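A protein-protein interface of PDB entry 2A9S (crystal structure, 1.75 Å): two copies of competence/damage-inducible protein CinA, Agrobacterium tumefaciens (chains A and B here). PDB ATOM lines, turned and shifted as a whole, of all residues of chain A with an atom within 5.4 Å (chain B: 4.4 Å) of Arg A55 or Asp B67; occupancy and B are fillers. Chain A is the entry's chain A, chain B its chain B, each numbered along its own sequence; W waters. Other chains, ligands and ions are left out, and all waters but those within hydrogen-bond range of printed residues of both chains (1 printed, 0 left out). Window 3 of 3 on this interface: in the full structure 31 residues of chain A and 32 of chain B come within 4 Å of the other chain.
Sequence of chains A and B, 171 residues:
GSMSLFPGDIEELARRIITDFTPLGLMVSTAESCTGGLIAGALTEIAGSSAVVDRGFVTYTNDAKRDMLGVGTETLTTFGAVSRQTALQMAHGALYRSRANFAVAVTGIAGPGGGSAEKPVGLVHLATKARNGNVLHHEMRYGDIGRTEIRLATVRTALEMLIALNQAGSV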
ATOM      1  N   VAL A  28     -17.020 -11.710  16.898  1.00  0.00           N
ATOM      2  CA  VAL A  28     -16.216 -10.618  17.423  1.00  0.00           C
ATOM      3  C   VAL A  28     -15.089 -11.156  18.302  1.00  0.00           C
ATOM      4  O   VAL A  28     -15.248 -12.198  18.966  1.00  0.00           O
ATOM      5  CB  VAL A  28     -17.089  -9.615  18.245  1.00  0.00           C
ATOM      6  CG1 VAL A  28     -17.797 -10.314  19.397  1.00  0.00           C
ATOM      7  CG2 VAL A  28     -16.242  -8.414  18.740  1.00  0.00           C
ATOM      8  N   SER A  29     -13.981 -10.441  18.318  1.00  0.00           N
ATOM      9  CA  SER A  29     -12.945 -10.696  19.308  1.00  0.00           C
ATOM     10  C   SER A  29     -12.605  -9.389  19.980  1.00  0.00           C
ATOM     11  O   SER A  29     -12.823  -8.321  19.415  1.00  0.00           O
ATOM     12  CB  SER A  29     -11.703 -11.324  18.686  1.00  0.00           C
ATOM     13  OG  SER A  29     -11.097 -10.462  17.754  1.00  0.00           O
ATOM     14  N   THR A  30     -12.092  -9.483  21.200  1.00  0.00           N
ATOM     15  CA  THR A  30     -11.842  -8.277  21.973  1.00  0.00           C
ATOM     16  C   THR A  30     -10.407  -8.308  22.415  1.00  0.00           C
ATOM     17  O   THR A  30      -9.858  -9.391  22.675  1.00  0.00           O
ATOM     18  CB  THR A  30     -12.791  -8.219  23.225  1.00  0.00           C
ATOM     19  OG1 THR A  30     -12.512  -9.317  24.090  1.00  0.00           O
ATOM     20  CG2 THR A  30     -14.275  -8.366  22.789  1.00  0.00           C
ATOM     21  N   VAL A  53     -19.269 -14.463  20.147  1.00  0.00           N
ATOM     22  CA  VAL A  53     -18.009 -14.088  20.759  1.00  0.00           C
ATOM     23  C   VAL A  53     -16.968 -15.185  20.496  1.00  0.00           C
ATOM     24  O   VAL A  53     -17.119 -16.322  20.946  1.00  0.00           O
ATOM     25  CB  VAL A  53     -18.167 -13.771  22.265  1.00  0.00           C
ATOM     26  CG1 VAL A  53     -16.818 -13.381  22.837  1.00  0.00           C
ATOM     27  CG2 VAL A  53     -19.147 -12.651  22.496  1.00  0.00           C
ATOM     28  N   ASP A  54     -15.929 -14.848  19.754  1.00  0.00           N
ATOM     29  CA  ASP A  54     -14.950 -15.844  19.357  1.00  0.00           C
ATOM     30  C   ASP A  54     -13.907 -16.024  20.446  1.00  0.00           C
ATOM     31  O   ASP A  54     -13.805 -17.116  21.020  1.00  0.00           O
ATOM     32  CB  ASP A  54     -14.330 -15.481  18.026  1.00  0.00           C
ATOM     33  CG  ASP A  54     -13.340 -16.540  17.530  1.00  0.00           C
ATOM     34  OD1 ASP A  54     -13.778 -17.704  17.362  1.00  0.00           O
ATOM     35  OD2 ASP A  54     -12.158 -16.192  17.317  1.00  0.00           O
ATOM     36  N   ARG A  55     -13.166 -14.967  20.747  1.00  0.00           N
ATOM     37  CA  ARG A  55     -12.185 -15.036  21.832  1.00  0.00           C
ATOM     38  C   ARG A  55     -11.851 -13.650  22.311  1.00  0.00           C
ATOM     39  O   ARG A  55     -12.202 -12.650  21.677  1.00  0.00           O
ATOM     40  CB  ARG A  55     -10.902 -15.771  21.389  1.00  0.00           C
ATOM     41  CG  ARG A  55     -10.144 -15.035  20.288  1.00  0.00           C
ATOM     42  CD  ARG A  55      -9.077 -15.919  19.639  1.00  0.00           C
ATOM     43  NE  ARG A  55      -9.680 -17.024  18.912  1.00  0.00           N
ATOM     44  CZ  ARG A  55      -9.012 -18.076  18.445  1.00  0.00           C
ATOM     45  NH1 ARG A  55      -7.681 -18.200  18.617  1.00  0.00           N
ATOM     46  NH2 ARG A  55      -9.676 -19.009  17.813  1.00  0.00           N
ATOM     47  N   GLY A  56     -11.151 -13.588  23.429  1.00  0.00           N
ATOM     48  CA  GLY A  56     -10.789 -12.318  24.025  1.00  0.00           C
ATOM     49  C   GLY A  56      -9.379 -12.390  24.545  1.00  0.00           C
ATOM     50  O   GLY A  56      -8.960 -13.453  25.055  1.00  0.00           O
ATOM     51  N   PHE A  57      -8.669 -11.255  24.443  1.00  0.00           N
ATOM     52  CA  PHE A  57      -7.289 -11.122  24.941  1.00  0.00           C
ATOM     53  C   PHE A  57      -7.292 -10.017  25.969  1.00  0.00           C
ATOM     54  O   PHE A  57      -7.765  -8.919  25.673  1.00  0.00           O
ATOM     55  CB  PHE A  57      -6.367 -10.714  23.802  1.00  0.00           C
ATOM     56  CG  PHE A  57      -6.456 -11.607  22.577  1.00  0.00           C
ATOM     57  CD1 PHE A  57      -5.581 -12.678  22.449  1.00  0.00           C
ATOM     58  CD2 PHE A  57      -7.403 -11.387  21.576  1.00  0.00           C
ATOM     59  CE1 PHE A  57      -5.634 -13.515  21.331  1.00  0.00           C
ATOM     60  CE2 PHE A  57      -7.470 -12.227  20.469  1.00  0.00           C
ATOM     61  CZ  PHE A  57      -6.594 -13.281  20.351  1.00  0.00           C
ATOM     62  N   ARG A  97      -5.401 -12.893  14.758  1.00  0.00           N
ATOM     63  CA  ARG A  97      -5.157 -14.037  15.641  1.00  0.00           C
ATOM     64  C   ARG A  97      -6.473 -14.638  16.196  1.00  0.00           C
ATOM     65  O   ARG A  97      -6.517 -15.205  17.305  1.00  0.00           O
ATOM     66  CB  ARG A  97      -4.155 -13.689  16.737  1.00  0.00           C
ATOM     67  CG  ARG A  97      -2.762 -13.440  16.158  1.00  0.00           C
ATOM     68  CD  ARG A  97      -1.825 -12.820  17.138  1.00  0.00           C
ATOM     69  NE  ARG A  97      -0.562 -12.385  16.514  1.00  0.00           N
ATOM     70  CZ  ARG A  97       0.626 -12.418  17.120  1.00  0.00           C
ATOM     71  NH1 ARG A  97       0.756 -12.901  18.349  1.00  0.00           N
ATOM     72  NH2 ARG A  97       1.700 -11.980  16.488  1.00  0.00           N
ATOM     73  N   SER A  98      -7.543 -14.514  15.407  1.00  0.00           N
ATOM     74  CA  SER A  98      -8.836 -15.072  15.766  1.00  0.00           C
ATOM     75  C   SER A  98      -9.598 -15.471  14.517  1.00  0.00           C
ATOM     76  O   SER A  98      -9.099 -15.257  13.392  1.00  0.00           O
ATOM     77  CB  SER A  98      -9.646 -14.057  16.571  1.00  0.00           C
ATOM     78  OG  SER A  98     -10.305 -13.128  15.726  1.00  0.00           O
ATOM     79  N   ARG A  99     -10.795 -16.021  14.718  1.00  0.00           N
ATOM     80  CA  ARG A  99     -11.698 -16.342  13.624  1.00  0.00           C
ATOM     81  C   ARG A  99     -12.803 -15.310  13.514  1.00  0.00           C
ATOM     82  O   ARG A  99     -13.774 -15.540  12.810  1.00  0.00           O
ATOM     83  CB  ARG A  99     -12.321 -17.742  13.812  1.00  0.00           C
ATOM     84  CG  ARG A  99     -11.346 -18.781  14.281  1.00  0.00           C
ATOM     85  CD  ARG A  99     -11.901 -20.165  14.053  1.00  0.00           C
ATOM     86  NE  ARG A  99     -10.848 -21.068  13.589  1.00  0.00           N
ATOM     87  CZ  ARG A  99     -10.706 -21.470  12.327  1.00  0.00           C
ATOM     88  NH1 ARG A  99     -11.561 -21.075  11.384  1.00  0.00           N
ATOM     89  NH2 ARG A  99      -9.705 -22.283  12.011  1.00  0.00           N
ATOM     90  N   VAL B  58      -9.564 -15.355  27.066  1.00  0.00           N
ATOM     91  CA  VAL B  58     -10.977 -15.675  27.070  1.00  0.00           C
ATOM     92  C   VAL B  58     -11.264 -16.606  25.881  1.00  0.00           C
ATOM     93  O   VAL B  58     -11.211 -16.175  24.738  1.00  0.00           O
ATOM     94  CB  VAL B  58     -11.854 -14.397  27.057  1.00  0.00           C
ATOM     95  CG1 VAL B  58     -13.324 -14.778  27.125  1.00  0.00           C
ATOM     96  CG2 VAL B  58     -11.474 -13.482  28.259  1.00  0.00           C
ATOM     97  N   TYR B  60     -13.954 -19.191  24.873  1.00  0.00           N
ATOM     98  CA  TYR B  60     -15.266 -19.842  24.847  1.00  0.00           C
ATOM     99  C   TYR B  60     -15.254 -21.010  23.892  1.00  0.00           C
ATOM    100  O   TYR B  60     -15.685 -22.116  24.219  1.00  0.00           O
ATOM    101  CB  TYR B  60     -16.302 -18.864  24.330  1.00  0.00           C
ATOM    102  CG  TYR B  60     -15.937 -17.421  24.522  1.00  0.00           C
ATOM    103  CD1 TYR B  60     -16.613 -16.648  25.453  1.00  0.00           C
ATOM    104  CD2 TYR B  60     -14.909 -16.836  23.791  1.00  0.00           C
ATOM    105  CE1 TYR B  60     -16.322 -15.356  25.639  1.00  0.00           C
ATOM    106  CE2 TYR B  60     -14.586 -15.531  23.977  1.00  0.00           C
ATOM    107  CZ  TYR B  60     -15.300 -14.786  24.912  1.00  0.00           C
ATOM    108  OH  TYR B  60     -15.001 -13.471  25.108  1.00  0.00           O
ATOM    109  N   ASP B  63     -11.858 -24.188  19.699  1.00  0.00           N
ATOM    110  CA  ASP B  63     -10.735 -23.815  18.856  1.00  0.00           C
ATOM    111  C   ASP B  63      -9.828 -22.864  19.629  1.00  0.00           C
ATOM    112  O   ASP B  63      -8.602 -22.975  19.539  1.00  0.00           O
ATOM    113  CB  ASP B  63     -11.193 -23.141  17.554  1.00  0.00           C
ATOM    114  CG  ASP B  63     -10.035 -22.790  16.669  1.00  0.00           C
ATOM    115  OD1 ASP B  63      -9.411 -23.725  16.138  1.00  0.00           O
ATOM    116  OD2 ASP B  63      -9.704 -21.593  16.550  1.00  0.00           O
ATOM    117  N   ALA B  64     -10.421 -21.935  20.389  1.00  0.00           N
ATOM    118  CA  ALA B  64      -9.636 -20.972  21.150  1.00  0.00           C
ATOM    119  C   ALA B  64      -8.893 -21.656  22.279  1.00  0.00           C
ATOM    120  O   ALA B  64      -7.773 -21.271  22.584  1.00  0.00           O
ATOM    121  CB  ALA B  64     -10.523 -19.822  21.725  1.00  0.00           C
ATOM    122  N   LYS B  65      -9.524 -22.642  22.926  1.00  0.00           N
ATOM    123  CA  LYS B  65      -8.846 -23.389  23.965  1.00  0.00           C
ATOM    124  C   LYS B  65      -7.621 -24.072  23.407  1.00  0.00           C
ATOM    125  O   LYS B  65      -6.545 -24.010  24.007  1.00  0.00           O
ATOM    126  CB  LYS B  65      -9.774 -24.430  24.585  1.00  0.00           C
ATOM    127  CG  LYS B  65     -10.925 -23.828  25.384  1.00  0.00           C
ATOM    128  CD  LYS B  65     -11.753 -24.977  25.922  1.00  0.00           C
ATOM    129  CE  LYS B  65     -12.948 -24.500  26.752  1.00  0.00           C
ATOM    130  NZ  LYS B  65     -13.913 -23.699  25.930  1.00  0.00           N
ATOM    131  N   ARG B  66      -7.774 -24.730  22.263  1.00  0.00           N
ATOM    132  CA  ARG B  66      -6.610 -25.388  21.650  1.00  0.00           C
ATOM    133  C   ARG B  66      -5.529 -24.373  21.183  1.00  0.00           C
ATOM    134  O   ARG B  66      -4.339 -24.496  21.550  1.00  0.00           O
ATOM    135  CB  ARG B  66      -7.074 -26.296  20.504  1.00  0.00           C
ATOM    136  CG  ARG B  66      -5.945 -27.100  19.844  1.00  0.00           C
ATOM    137  CD  ARG B  66      -6.548 -28.006  18.765  1.00  0.00           C
ATOM    138  NE  ARG B  66      -7.289 -27.216  17.782  1.00  0.00           N
ATOM    139  CZ  ARG B  66      -8.091 -27.732  16.858  1.00  0.00           C
ATOM    140  NH1 ARG B  66      -8.247 -29.049  16.775  1.00  0.00           N
ATOM    141  NH2 ARG B  66      -8.720 -26.919  16.010  1.00  0.00           N
ATOM    142  N   ASP B  67      -5.959 -23.371  20.411  1.00  0.00           N
ATOM    143  CA  ASP B  67      -5.076 -22.361  19.776  1.00  0.00           C
ATOM    144  C   ASP B  67      -4.324 -21.506  20.805  1.00  0.00           C
ATOM    145  O   ASP B  67      -3.089 -21.362  20.748  1.00  0.00           O
ATOM    146  CB  ASP B  67      -5.891 -21.490  18.780  1.00  0.00           C
ATOM    147  CG  ASP B  67      -5.035 -20.442  18.063  1.00  0.00           C
ATOM    148  OD1 ASP B  67      -3.806 -20.613  17.997  1.00  0.00           O
ATOM    149  OD2 ASP B  67      -5.567 -19.438  17.539  1.00  0.00           O
ATOM    150  N   MET B  68      -5.041 -21.000  21.798  1.00  0.00           N
ATOM    151  CA  MET B  68      -4.465 -20.021  22.724  1.00  0.00           C
ATOM    152  C   MET B  68      -3.797 -20.705  23.920  1.00  0.00           C
ATOM    153  O   MET B  68      -2.835 -20.183  24.449  1.00  0.00           O
ATOM    154  CB  MET B  68      -5.571 -19.057  23.225  1.00  0.00           C
ATOM    155  CG  MET B  68      -6.044 -18.077  22.145  1.00  0.00           C
ATOM    156  SD  MET B  68      -7.545 -17.129  22.624  1.00  0.00           S
ATOM    157  CE  MET B  68      -7.040 -16.410  24.062  1.00  0.00           C
ATOM    158  N   LEU B  69      -4.305 -21.858  24.345  1.00  0.00           N
ATOM    159  CA  LEU B  69      -3.876 -22.484  25.616  1.00  0.00           C
ATOM    160  C   LEU B  69      -3.215 -23.868  25.470  1.00  0.00           C
ATOM    161  O   LEU B  69      -2.718 -24.450  26.452  1.00  0.00           O
ATOM    162  CB  LEU B  69      -5.049 -22.547  26.609  1.00  0.00           C
ATOM    163  CG  LEU B  69      -5.680 -21.210  27.006  1.00  0.00           C
ATOM    164  CD1 LEU B  69      -7.025 -21.471  27.781  1.00  0.00           C
ATOM    165  CD2 LEU B  69      -4.669 -20.369  27.816  1.00  0.00           C
ATOM    166  N   ARG B  97       2.201 -19.893  29.151  1.00  0.00           N
ATOM    167  CA  ARG B  97       2.107 -18.937  28.055  1.00  0.00           C
ATOM    168  C   ARG B  97       1.926 -17.521  28.593  1.00  0.00           C
ATOM    169  O   ARG B  97       1.373 -16.662  27.916  1.00  0.00           O
ATOM    170  CB  ARG B  97       0.977 -19.293  27.090  1.00  0.00           C
ATOM    171  CG  ARG B  97       1.239 -20.647  26.390  1.00  0.00           C
ATOM    172  CD  ARG B  97       0.098 -21.076  25.451  1.00  0.00           C
ATOM    173  NE  ARG B  97       0.377 -22.459  25.037  1.00  0.00           N
ATOM    174  CZ  ARG B  97       0.102 -22.990  23.837  1.00  0.00           C
ATOM    175  NH1 ARG B  97      -0.542 -22.277  22.900  1.00  0.00           N
ATOM    176  NH2 ARG B  97       0.468 -24.245  23.597  1.00  0.00           N
HETATM  177  O   HOH W   1     -12.251 -19.619  17.838  1.00  0.00           O
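OD2 of Asp B63 lies within salt-bridge range of NH2 of Arg A55, at 2.9 Å. The guanidinium group (NH1) of Arg A55 is in salt-bridge range of the side-chain carboxylate (OD2) of Asp B67 (2.7 Å). The backbone carbonyl oxygen (O) of Gly A56 lies within hydrogen-bond range of the backbone NH (N) of Val B58, at 2.8 Å. The guanidinium group (NE) of Arg A99 lies within salt-bridge range of the side-chain carboxylate (OD2) of Asp B63, at 3.2 Å.
Printed residues of chain A within 4 Å of Asp B67: Arg A55. Printed residues of chain A within 4 Å of Ala B64: Arg A55 (3.9 Å). Of the printed residues of chain B, Arg A99 touches Asp B63 (3.2 Å). Of the printed residues of chain A, Val B58 touches Arg A55 (3.3 Å) and Gly A56 (2.8 Å). Lys B65 touches none of the printed residues of chain A.
Water W1 lies within hydrogen-bond range of the side-chain carboxylate (OD1) of Asp A54 (2.5 Å), the guanidinium group (NH2) of Arg A55 (2.6 Å) and the side-chain carboxylate (OD2) of Asp B63 (3.5 Å).
Position printed for both chains: 97. Of the 12 pairs that touch across the chains among the printed residues, none has its exchanged pair printed and touching as well.
Val A53 touches Tyr B60. Tyr B60 touches Asp A54. CA of Arg A55 touches O of Val B58, 3.3 Å away. Arg A55 touches Tyr B60 (CA to CE2, 3.3 Å). Arg A55 touches Ala B64 (NH2 to CA, 3.9 Å). CD of Arg A55 touches SD of Met B68, at 3.6 Å. Gly A56 touches Tyr B60. Met B68 touches Gly A56.
The backbone carbonyl oxygen (O) of Val A28 is in hydrogen-bond range of the backbone NH (N) of Asp A54, at 2.8 Å. The guanidinium group of Arg A55 is in salt-bridge range of the side-chain carboxylate of Asp A54 (3.1 Å). NH1 of Arg A55 lies within hydrogen-bond range of O of Arg A97, 3.5 Å away. The backbone carbonyl oxygen (O) of Tyr B60 is in hydrogen-bond range of the side-chain amino group (NZ) of Lys B65 (2.9 Å). NH1 of Arg B97 is in hydrogen-bond range of O of Asp B67 (3.5 Å). The backbone carbonyl oxygen (O) of Met B68 lies close to the guanidinium group (NH1) of Arg B97.
Of the 11 printed residues of chain A, 5 touch a printed residue of chain B. Hydrophobic or aromatic side chains of chain A within 4 Å of the printed part of chain B: Val A53. Along chain A the printed residues that touch a printed residue of chain B span positions 53 to 99. Of the 10 printed residues of chain B, 6 touch a printed residue of chain A. Printed residues of chain B that touch a printed residue of chain A: Val B58, Tyr B60, Asp B63, Ala B64, Asp B67 and Met B68. Hydrophobic or aromatic side chains of chain B that line the printed part of chain A: Val B58, Tyr B60 and Met B68. Among the printed residues, Asp or Glu carboxylates within 4 Å of a Lys or Arg side-chain nitrogen of the other chain: Arg A55 with Asp B63 (2.9 Å), Arg A55 with Asp B67 (2.7 Å) and Arg A99 with Asp B63 (3.2 Å).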
